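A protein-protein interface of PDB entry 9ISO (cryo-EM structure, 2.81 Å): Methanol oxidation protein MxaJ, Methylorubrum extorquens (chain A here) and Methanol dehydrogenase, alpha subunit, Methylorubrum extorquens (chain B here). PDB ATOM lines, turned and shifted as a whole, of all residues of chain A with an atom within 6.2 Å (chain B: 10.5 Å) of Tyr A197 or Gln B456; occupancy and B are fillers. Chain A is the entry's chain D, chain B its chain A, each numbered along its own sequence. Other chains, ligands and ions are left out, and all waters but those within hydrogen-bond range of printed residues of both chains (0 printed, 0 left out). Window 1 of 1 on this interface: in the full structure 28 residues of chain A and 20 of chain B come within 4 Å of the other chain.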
ATOM      1  N   GLN A  60      21.949 -17.042 -16.629  1.00  0.00           N
ATOM      2  CA  GLN A  60      22.839 -16.726 -17.737  1.00  0.00           C
ATOM      3  C   GLN A  60      22.991 -15.216 -17.868  1.00  0.00           C
ATOM      4  O   GLN A  60      22.163 -14.561 -18.513  1.00  0.00           O
ATOM      5  CB  GLN A  60      22.307 -17.332 -19.035  1.00  0.00           C
ATOM      6  CG  GLN A  60      23.165 -17.058 -20.251  1.00  0.00           C
ATOM      7  CD  GLN A  60      23.163 -18.211 -21.227  1.00  0.00           C
ATOM      8  OE1 GLN A  60      22.866 -19.346 -20.859  1.00  0.00           O
ATOM      9  NE2 GLN A  60      23.491 -17.927 -22.481  1.00  0.00           N
ATOM     10  N   PRO A  95      22.433 -24.702 -18.176  1.00  0.00           N
ATOM     11  CA  PRO A  95      22.454 -23.478 -18.990  1.00  0.00           C
ATOM     12  C   PRO A  95      21.297 -23.388 -19.974  1.00  0.00           C
ATOM     13  O   PRO A  95      20.473 -24.303 -20.069  1.00  0.00           O
ATOM     14  CB  PRO A  95      23.802 -23.568 -19.715  1.00  0.00           C
ATOM     15  CG  PRO A  95      24.651 -24.388 -18.806  1.00  0.00           C
ATOM     16  CD  PRO A  95      23.728 -25.402 -18.202  1.00  0.00           C
ATOM     17  N   ILE A  97      20.906 -23.564 -23.183  1.00  0.00           N
ATOM     18  CA  ILE A  97      20.773 -24.481 -24.310  1.00  0.00           C
ATOM     19  C   ILE A  97      19.934 -25.698 -23.958  1.00  0.00           C
ATOM     20  O   ILE A  97      19.404 -26.364 -24.855  1.00  0.00           O
ATOM     21  CB  ILE A  97      22.168 -24.900 -24.822  1.00  0.00           C
ATOM     22  CG1 ILE A  97      22.099 -25.311 -26.293  1.00  0.00           C
ATOM     23  CG2 ILE A  97      22.743 -26.028 -23.981  1.00  0.00           C
ATOM     24  CD1 ILE A  97      23.410 -25.164 -27.024  1.00  0.00           C
ATOM     25  N   TYR A  98      19.787 -26.006 -22.672  1.00  0.00           N
ATOM     26  CA  TYR A  98      19.028 -27.164 -22.222  1.00  0.00           C
ATOM     27  C   TYR A  98      17.584 -26.826 -21.874  1.00  0.00           C
ATOM     28  O   TYR A  98      16.872 -27.688 -21.348  1.00  0.00           O
ATOM     29  CB  TYR A  98      19.712 -27.802 -21.011  1.00  0.00           C
ATOM     30  CG  TYR A  98      21.065 -28.403 -21.308  1.00  0.00           C
ATOM     31  CD1 TYR A  98      21.183 -29.540 -22.094  1.00  0.00           C
ATOM     32  CD2 TYR A  98      22.223 -27.838 -20.796  1.00  0.00           C
ATOM     33  CE1 TYR A  98      22.415 -30.093 -22.364  1.00  0.00           C
ATOM     34  CE2 TYR A  98      23.461 -28.385 -21.060  1.00  0.00           C
ATOM     35  CZ  TYR A  98      23.550 -29.512 -21.845  1.00  0.00           C
ATOM     36  OH  TYR A  98      24.782 -30.061 -22.112  1.00  0.00           O
ATOM     37  N   TYR A 133      25.646  -9.939 -35.428  1.00  0.00           N
ATOM     38  CA  TYR A 133      26.980  -9.901 -34.851  1.00  0.00           C
ATOM     39  C   TYR A 133      27.629  -8.550 -35.119  1.00  0.00           C
ATOM     40  O   TYR A 133      27.381  -7.909 -36.143  1.00  0.00           O
ATOM     41  CB  TYR A 133      27.849 -11.025 -35.414  1.00  0.00           C
ATOM     42  CG  TYR A 133      27.575 -12.370 -34.790  1.00  0.00           C
ATOM     43  CD1 TYR A 133      26.583 -13.198 -35.289  1.00  0.00           C
ATOM     44  CD2 TYR A 133      28.303 -12.809 -33.696  1.00  0.00           C
ATOM     45  CE1 TYR A 133      26.325 -14.425 -34.718  1.00  0.00           C
ATOM     46  CE2 TYR A 133      28.053 -14.036 -33.119  1.00  0.00           C
ATOM     47  CZ  TYR A 133      27.064 -14.840 -33.633  1.00  0.00           C
ATOM     48  OH  TYR A 133      26.811 -16.064 -33.062  1.00  0.00           O
ATOM     49  N   PHE A 163      32.889 -20.126 -29.286  1.00  0.00           N
ATOM     50  CA  PHE A 163      32.901 -21.475 -29.835  1.00  0.00           C
ATOM     51  C   PHE A 163      31.564 -21.808 -30.486  1.00  0.00           C
ATOM     52  O   PHE A 163      30.505 -21.357 -30.043  1.00  0.00           O
ATOM     53  CB  PHE A 163      33.214 -22.506 -28.748  1.00  0.00           C
ATOM     54  CG  PHE A 163      34.565 -22.334 -28.119  1.00  0.00           C
ATOM     55  CD1 PHE A 163      35.707 -22.294 -28.897  1.00  0.00           C
ATOM     56  CD2 PHE A 163      34.692 -22.207 -26.750  1.00  0.00           C
ATOM     57  CE1 PHE A 163      36.948 -22.132 -28.319  1.00  0.00           C
ATOM     58  CE2 PHE A 163      35.930 -22.043 -26.170  1.00  0.00           C
ATOM     59  CZ  PHE A 163      37.057 -22.007 -26.955  1.00  0.00           C
ATOM     60  N   GLY A 164      31.625 -22.612 -31.543  1.00  0.00           N
ATOM     61  CA  GLY A 164      30.422 -22.975 -32.277  1.00  0.00           C
ATOM     62  C   GLY A 164      29.728 -21.791 -32.912  1.00  0.00           C
ATOM     63  O   GLY A 164      28.493 -21.732 -32.930  1.00  0.00           O
ATOM     64  N   THR A 165      30.497 -20.853 -33.449  1.00  0.00           N
ATOM     65  CA  THR A 165      29.999 -19.590 -33.960  1.00  0.00           C
ATOM     66  C   THR A 165      30.492 -19.399 -35.387  1.00  0.00           C
ATOM     67  O   THR A 165      31.577 -19.875 -35.736  1.00  0.00           O
ATOM     68  CB  THR A 165      30.485 -18.433 -33.067  1.00  0.00           C
ATOM     69  OG1 THR A 165      30.029 -18.647 -31.726  1.00  0.00           O
ATOM     70  CG2 THR A 165      29.977 -17.082 -33.548  1.00  0.00           C
ATOM     71  N   PRO A 166      29.712 -18.727 -36.238  1.00  0.00           N
ATOM     72  CA  PRO A 166      30.206 -18.410 -37.588  1.00  0.00           C
ATOM     73  C   PRO A 166      31.513 -17.635 -37.600  1.00  0.00           C
ATOM     74  O   PRO A 166      32.238 -17.693 -38.602  1.00  0.00           O
ATOM     75  CB  PRO A 166      29.062 -17.587 -38.186  1.00  0.00           C
ATOM     76  CG  PRO A 166      27.852 -18.132 -37.529  1.00  0.00           C
ATOM     77  CD  PRO A 166      28.255 -18.536 -36.133  1.00  0.00           C
ATOM     78  N   PRO A 193      35.020 -30.278 -21.800  1.00  0.00           N
ATOM     79  CA  PRO A 193      34.649 -31.677 -22.025  1.00  0.00           C
ATOM     80  C   PRO A 193      33.752 -31.833 -23.243  1.00  0.00           C
ATOM     81  O   PRO A 193      33.005 -30.926 -23.617  1.00  0.00           O
ATOM     82  CB  PRO A 193      33.908 -32.065 -20.739  1.00  0.00           C
ATOM     83  CG  PRO A 193      34.211 -30.979 -19.756  1.00  0.00           C
ATOM     84  CD  PRO A 193      34.437 -29.748 -20.559  1.00  0.00           C
ATOM     85  N   ASN A 195      31.218 -33.793 -23.526  1.00  0.00           N
ATOM     86  CA  ASN A 195      29.835 -34.072 -23.170  1.00  0.00           C
ATOM     87  C   ASN A 195      29.171 -32.916 -22.434  1.00  0.00           C
ATOM     88  O   ASN A 195      28.022 -33.051 -22.000  1.00  0.00           O
ATOM     89  CB  ASN A 195      29.750 -35.345 -22.324  1.00  0.00           C
ATOM     90  CG  ASN A 195      30.742 -35.351 -21.178  1.00  0.00           C
ATOM     91  OD1 ASN A 195      31.501 -34.400 -20.992  1.00  0.00           O
ATOM     92  ND2 ASN A 195      30.740 -36.426 -20.402  1.00  0.00           N
ATOM     93  N   GLN A 196      29.857 -31.788 -22.279  1.00  0.00           N
ATOM     94  CA  GLN A 196      29.317 -30.655 -21.545  1.00  0.00           C
ATOM     95  C   GLN A 196      29.582 -29.379 -22.331  1.00  0.00           C
ATOM     96  O   GLN A 196      30.592 -29.262 -23.029  1.00  0.00           O
ATOM     97  CB  GLN A 196      29.922 -30.576 -20.135  1.00  0.00           C
ATOM     98  CG  GLN A 196      29.219 -29.613 -19.191  1.00  0.00           C
ATOM     99  CD  GLN A 196      29.802 -28.216 -19.239  1.00  0.00           C
ATOM    100  OE1 GLN A 196      30.990 -28.036 -19.502  1.00  0.00           O
ATOM    101  NE2 GLN A 196      28.966 -27.216 -18.984  1.00  0.00           N
ATOM    102  N   TYR A 197      28.665 -28.424 -22.210  1.00  0.00           N
ATOM    103  CA  TYR A 197      28.688 -27.198 -22.998  1.00  0.00           C
ATOM    104  C   TYR A 197      29.506 -26.129 -22.288  1.00  0.00           C
ATOM    105  O   TYR A 197      29.284 -25.854 -21.104  1.00  0.00           O
ATOM    106  CB  TYR A 197      27.265 -26.697 -23.249  1.00  0.00           C
ATOM    107  CG  TYR A 197      27.188 -25.292 -23.798  1.00  0.00           C
ATOM    108  CD1 TYR A 197      27.427 -25.038 -25.140  1.00  0.00           C
ATOM    109  CD2 TYR A 197      26.870 -24.222 -22.976  1.00  0.00           C
ATOM    110  CE1 TYR A 197      27.358 -23.756 -25.647  1.00  0.00           C
ATOM    111  CE2 TYR A 197      26.799 -22.937 -23.473  1.00  0.00           C
ATOM    112  CZ  TYR A 197      27.044 -22.710 -24.808  1.00  0.00           C
ATOM    113  OH  TYR A 197      26.973 -21.432 -25.308  1.00  0.00           O
ATOM    114  N   THR A 198      30.444 -25.523 -23.016  1.00  0.00           N
ATOM    115  CA  THR A 198      31.278 -24.447 -22.501  1.00  0.00           C
ATOM    116  C   THR A 198      31.250 -23.266 -23.461  1.00  0.00           C
ATOM    117  O   THR A 198      31.086 -23.436 -24.672  1.00  0.00           O
ATOM    118  CB  THR A 198      32.729 -24.901 -22.293  1.00  0.00           C
ATOM    119  OG1 THR A 198      33.288 -25.305 -23.549  1.00  0.00           O
ATOM    120  CG2 THR A 198      32.798 -26.055 -21.314  1.00  0.00           C
ATOM    121  N   GLN A 199      31.415 -22.067 -22.910  1.00  0.00           N
ATOM    122  CA  GLN A 199      31.406 -20.850 -23.709  1.00  0.00           C
ATOM    123  C   GLN A 199      32.082 -19.735 -22.925  1.00  0.00           C
ATOM    124  O   GLN A 199      32.041 -19.714 -21.692  1.00  0.00           O
ATOM    125  CB  GLN A 199      29.979 -20.447 -24.098  1.00  0.00           C
ATOM    126  CG  GLN A 199      29.893 -19.260 -25.043  1.00  0.00           C
ATOM    127  CD  GLN A 199      30.649 -19.486 -26.333  1.00  0.00           C
ATOM    128  OE1 GLN A 199      31.648 -18.823 -26.603  1.00  0.00           O
ATOM    129  NE2 GLN A 199      30.173 -20.424 -27.141  1.00  0.00           N
ATOM    130  N   PHE B 448      25.708 -36.562 -30.464  1.00  0.00           N
ATOM    131  CA  PHE B 448      24.535 -35.701 -30.454  1.00  0.00           C
ATOM    132  C   PHE B 448      24.907 -34.300 -30.917  1.00  0.00           C
ATOM    133  O   PHE B 448      26.074 -33.894 -30.875  1.00  0.00           O
ATOM    134  CB  PHE B 448      23.881 -35.656 -29.068  1.00  0.00           C
ATOM    135  CG  PHE B 448      24.790 -35.184 -27.974  1.00  0.00           C
ATOM    136  CD1 PHE B 448      24.883 -33.841 -27.664  1.00  0.00           C
ATOM    137  CD2 PHE B 448      25.534 -36.086 -27.240  1.00  0.00           C
ATOM    138  CE1 PHE B 448      25.711 -33.407 -26.656  1.00  0.00           C
ATOM    139  CE2 PHE B 448      26.366 -35.655 -26.229  1.00  0.00           C
ATOM    140  CZ  PHE B 448      26.453 -34.316 -25.938  1.00  0.00           C
ATOM    141  N   MET B 449      23.883 -33.569 -31.355  1.00  0.00           N
ATOM    142  CA  MET B 449      23.999 -32.191 -31.811  1.00  0.00           C
ATOM    143  C   MET B 449      22.808 -31.410 -31.278  1.00  0.00           C
ATOM    144  O   MET B 449      21.669 -31.873 -31.378  1.00  0.00           O
ATOM    145  CB  MET B 449      24.055 -32.125 -33.344  1.00  0.00           C
ATOM    146  CG  MET B 449      24.242 -30.733 -33.937  1.00  0.00           C
ATOM    147  SD  MET B 449      22.731 -29.755 -34.072  1.00  0.00           S
ATOM    148  CE  MET B 449      21.903 -30.596 -35.418  1.00  0.00           C
ATOM    149  N   LEU B 450      23.070 -30.232 -30.717  1.00  0.00           N
ATOM    150  CA  LEU B 450      22.029 -29.395 -30.124  1.00  0.00           C
ATOM    151  C   LEU B 450      22.095 -27.998 -30.724  1.00  0.00           C
ATOM    152  O   LEU B 450      23.162 -27.355 -30.674  1.00  0.00           O
ATOM    153  CB  LEU B 450      22.177 -29.333 -28.603  1.00  0.00           C
ATOM    154  CG  LEU B 450      21.954 -30.632 -27.837  1.00  0.00           C
ATOM    155  CD1 LEU B 450      22.272 -30.440 -26.367  1.00  0.00           C
ATOM    156  CD2 LEU B 450      20.527 -31.115 -28.020  1.00  0.00           C
ATOM    157  N   PRO B 451      21.008 -27.485 -31.291  1.00  0.00           N
ATOM    158  CA  PRO B 451      21.027 -26.134 -31.859  1.00  0.00           C
ATOM    159  C   PRO B 451      20.899 -25.068 -30.778  1.00  0.00           C
ATOM    160  O   PRO B 451      20.652 -25.350 -29.606  1.00  0.00           O
ATOM    161  CB  PRO B 451      19.807 -26.118 -32.791  1.00  0.00           C
ATOM    162  CG  PRO B 451      19.318 -27.538 -32.854  1.00  0.00           C
ATOM    163  CD  PRO B 451      19.750 -28.182 -31.584  1.00  0.00           C
ATOM    164  N   TYR B 452      21.072 -23.822 -31.203  1.00  0.00           N
ATOM    165  CA  TYR B 452      20.928 -22.673 -30.314  1.00  0.00           C
ATOM    166  C   TYR B 452      20.434 -21.493 -31.148  1.00  0.00           C
ATOM    167  O   TYR B 452      19.925 -21.674 -32.259  1.00  0.00           O
ATOM    168  CB  TYR B 452      22.243 -22.404 -29.567  1.00  0.00           C
ATOM    169  CG  TYR B 452      22.074 -21.545 -28.337  1.00  0.00           C
ATOM    170  CD1 TYR B 452      21.217 -21.925 -27.316  1.00  0.00           C
ATOM    171  CD2 TYR B 452      22.775 -20.357 -28.191  1.00  0.00           C
ATOM    172  CE1 TYR B 452      21.056 -21.145 -26.192  1.00  0.00           C
ATOM    173  CE2 TYR B 452      22.623 -19.572 -27.068  1.00  0.00           C
ATOM    174  CZ  TYR B 452      21.761 -19.971 -26.072  1.00  0.00           C
ATOM    175  OH  TYR B 452      21.604 -19.194 -24.950  1.00  0.00           O
ATOM    176  N   ARG B 453      20.579 -20.279 -30.614  1.00  0.00           N
ATOM    177  CA  ARG B 453      19.885 -19.110 -31.141  1.00  0.00           C
ATOM    178  C   ARG B 453      20.368 -18.667 -32.517  1.00  0.00           C
ATOM    179  O   ARG B 453      19.613 -18.734 -33.490  1.00  0.00           O
ATOM    180  CB  ARG B 453      20.024 -17.942 -30.163  1.00  0.00           C
ATOM    181  CG  ARG B 453      19.332 -18.152 -28.832  1.00  0.00           C
ATOM    182  CD  ARG B 453      19.480 -16.929 -27.946  1.00  0.00           C
ATOM    183  NE  ARG B 453      18.222 -16.211 -27.791  1.00  0.00           N
ATOM    184  CZ  ARG B 453      18.071 -15.113 -27.065  1.00  0.00           C
ATOM    185  NH1 ARG B 453      19.086 -14.575 -26.408  1.00  0.00           N
ATOM    186  NH2 ARG B 453      16.874 -14.540 -26.995  1.00  0.00           N
ATOM    187  N   ALA B 454      21.617 -18.225 -32.621  1.00  0.00           N
ATOM    188  CA  ALA B 454      22.098 -17.533 -33.814  1.00  0.00           C
ATOM    189  C   ALA B 454      23.140 -18.400 -34.515  1.00  0.00           C
ATOM    190  O   ALA B 454      24.346 -18.230 -34.332  1.00  0.00           O
ATOM    191  CB  ALA B 454      22.663 -16.164 -33.440  1.00  0.00           C
ATOM    192  N   GLY B 455      22.659 -19.327 -35.340  1.00  0.00           N
ATOM    193  CA  GLY B 455      23.543 -20.184 -36.113  1.00  0.00           C
ATOM    194  C   GLY B 455      24.524 -20.973 -35.279  1.00  0.00           C
ATOM    195  O   GLY B 455      25.591 -21.350 -35.777  1.00  0.00           O
ATOM    196  N   GLN B 456      24.195 -21.236 -34.021  1.00  0.00           N
ATOM    197  CA  GLN B 456      25.109 -21.860 -33.078  1.00  0.00           C
ATOM    198  C   GLN B 456      24.630 -23.268 -32.767  1.00  0.00           C
ATOM    199  O   GLN B 456      23.481 -23.460 -32.358  1.00  0.00           O
ATOM    200  CB  GLN B 456      25.211 -21.037 -31.793  1.00  0.00           C
ATOM    201  CG  GLN B 456      26.212 -21.577 -30.792  1.00  0.00           C
ATOM    202  CD  GLN B 456      26.331 -20.706 -29.558  1.00  0.00           C
ATOM    203  OE1 GLN B 456      25.634 -19.701 -29.424  1.00  0.00           O
ATOM    204  NE2 GLN B 456      27.218 -21.090 -28.648  1.00  0.00           N
ATOM    205  N   PHE B 457      25.507 -24.246 -32.967  1.00  0.00           N
ATOM    206  CA  PHE B 457      25.199 -25.628 -32.645  1.00  0.00           C
ATOM    207  C   PHE B 457      26.355 -26.239 -31.871  1.00  0.00           C
ATOM    208  O   PHE B 457      27.510 -25.836 -32.023  1.00  0.00           O
ATOM    209  CB  PHE B 457      24.886 -26.456 -33.909  1.00  0.00           C
ATOM    210  CG  PHE B 457      26.038 -26.581 -34.864  1.00  0.00           C
ATOM    211  CD1 PHE B 457      26.225 -25.647 -35.869  1.00  0.00           C
ATOM    212  CD2 PHE B 457      26.923 -27.644 -34.774  1.00  0.00           C
ATOM    213  CE1 PHE B 457      27.280 -25.761 -36.754  1.00  0.00           C
ATOM    214  CE2 PHE B 457      27.979 -27.763 -35.656  1.00  0.00           C
ATOM    215  CZ  PHE B 457      28.156 -26.820 -36.647  1.00  0.00           C
ATOM    216  N   PHE B 458      26.023 -27.210 -31.026  1.00  0.00           N
ATOM    217  CA  PHE B 458      26.982 -27.889 -30.168  1.00  0.00           C
ATOM    218  C   PHE B 458      26.987 -29.366 -30.527  1.00  0.00           C
ATOM    219  O   PHE B 458      25.956 -30.035 -30.417  1.00  0.00           O
ATOM    220  CB  PHE B 458      26.623 -27.691 -28.695  1.00  0.00           C
ATOM    221  CG  PHE B 458      27.422 -28.540 -27.753  1.00  0.00           C
ATOM    222  CD1 PHE B 458      28.717 -28.189 -27.412  1.00  0.00           C
ATOM    223  CD2 PHE B 458      26.874 -29.682 -27.194  1.00  0.00           C
ATOM    224  CE1 PHE B 458      29.452 -28.967 -26.540  1.00  0.00           C
ATOM    225  CE2 PHE B 458      27.604 -30.463 -26.322  1.00  0.00           C
ATOM    226  CZ  PHE B 458      28.894 -30.106 -25.993  1.00  0.00           C
ATOM    227  N   VAL B 459      28.142 -29.864 -30.961  1.00  0.00           N
ATOM    228  CA  VAL B 459      28.326 -31.270 -31.300  1.00  0.00           C
ATOM    229  C   VAL B 459      29.126 -31.933 -30.192  1.00  0.00           C
ATOM    230  O   VAL B 459      30.114 -31.372 -29.702  1.00  0.00           O
ATOM    231  CB  VAL B 459      29.021 -31.436 -32.665  1.00  0.00           C
ATOM    232  CG1 VAL B 459      28.069 -31.077 -33.788  1.00  0.00           C
ATOM    233  CG2 VAL B 459      30.267 -30.572 -32.737  1.00  0.00           C
ATOM    234  N   GLY B 460      28.695 -33.120 -29.780  1.00  0.00           N
ATOM    235  CA  GLY B 460      29.382 -33.786 -28.693  1.00  0.00           C
ATOM    236  C   GLY B 460      29.100 -35.269 -28.688  1.00  0.00           C
ATOM    237  O   GLY B 460      28.343 -35.787 -29.513  1.00  0.00           O
ATOM    238  N   ALA B 461      29.723 -35.953 -27.733  1.00  0.00           N
ATOM    239  CA  ALA B 461      29.583 -37.393 -27.594  1.00  0.00           C
ATOM    240  C   ALA B 461      29.517 -37.761 -26.122  1.00  0.00           C
ATOM    241  O   ALA B 461      30.303 -37.256 -25.317  1.00  0.00           O
ATOM    242  CB  ALA B 461      30.745 -38.129 -28.269  1.00  0.00           C
ATOM    243  N   THR B 462      28.579 -38.636 -25.779  1.00  0.00           N
ATOM    244  CA  THR B 462      28.471 -39.209 -24.446  1.00  0.00           C
ATOM    245  C   THR B 462      29.023 -40.626 -24.479  1.00  0.00           C
ATOM    246  O   THR B 462      28.610 -41.442 -25.311  1.00  0.00           O
ATOM    247  CB  THR B 462      27.020 -39.216 -23.965  1.00  0.00           C
ATOM    248  OG1 THR B 462      26.565 -37.869 -23.794  1.00  0.00           O
ATOM    249  CG2 THR B 462      26.899 -39.953 -22.646  1.00  0.00           C
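The side-chain amide nitrogen (NE2) of Gln A60 sits at hydrogen-bond distance from the side-chain hydroxyl (OH) of Tyr B452, 3.4 Å away.
The side-chain hydroxyl of Tyr A197 is in hydrogen-bond range of the side-chain amide nitrogen of Gln B456 (3.4 Å).
NE2 of Gln B456 lies close to NE2 of Gln A199.
The backbone carbonyl oxygen (O) of Leu B450 lies within hydrogen-bond range of the backbone NH (N) of Phe B458, 2.9 Å away.
The backbone carbonyl oxygen (O) of Phe A163 is in hydrogen-bond range of the side-chain hydroxyl (OG1) of Thr A165, at 3.2 Å.
O of Phe A163 sits at hydrogen-bond distance from NE2 of Gln A199 (3.1 Å).
Among the printed residues, pairs that only touch across the chains: Ile A97 with Pro B451 (3.6 Å), Ile A97 with Tyr B452 (3.6 Å), Tyr A133 with Ala B454 (3.5 Å), Phe A163 with Gln B456 (3.6 Å), Gly A164 with Gln B456 (3.1 Å), Gly A164 with Phe B457 (3.9 Å), Pro A166 with Gly B455 (3.9 Å), Asn A195 with Ala B461 (3.6 Å) and Gln A196 with Phe B458 (3.5 Å).
Of the printed residues of chain A, Gln B456 touches Phe A163 (3.6 Å), Gly A164 (3.1 Å), Tyr A197 (3.4 Å) and Gln A199 (3.4 Å).
Gln A196 touches just one residue of chain B: Phe B458.
Thr A198 touches none of the printed residues of chain B.
Of the printed residues of chain A, Gly B455 touches Pro A166 (3.9 Å).
Printed residues of chain A within 4 Å of Phe B457: Gly A164 (3.9 Å).
Of the printed residues of chain A, Pro B451 touches Ile A97 (3.6 Å).
The nearest residue of chain B that does not touch Tyr A197 is Phe B458 (4.03 Å).
The nearest residue of chain A that does not touch Gln B456 is Thr A165 (4.8 Å).
Of the 15 printed residues of chain B, 8 touch a printed residue of chain A.
Printed residues of chain B that touch a printed residue of chain A: Pro B451, Tyr B452, Ala B454, Gly B455, Gln B456, Phe B457, Phe B458 and Ala B461.
Hydrophobic or aromatic side chains of chain B within 4 Å of the printed part of chain A: Tyr B452 and Phe B458.
Of the 15 printed residues of chain A, 10 touch a printed residue of chain B.
Printed residues of chain A that touch a printed residue of chain B: Gln A60, Ile A97, Tyr A133, Phe A163, Gly A164, Pro A166, Asn A195, Gln A196, Tyr A197 and Gln A199.
Hydrophobic or aromatic side chains of chain A that line the printed part of chain B: Ile A97, Tyr A133, Pro A166 and Tyr A197.
Among the printed residues, 12 pairs touch across the chains.
Among the printed residues, no Asp or Glu carboxylate lies within 4 Å of a Lys or Arg side-chain nitrogen of the other chain.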
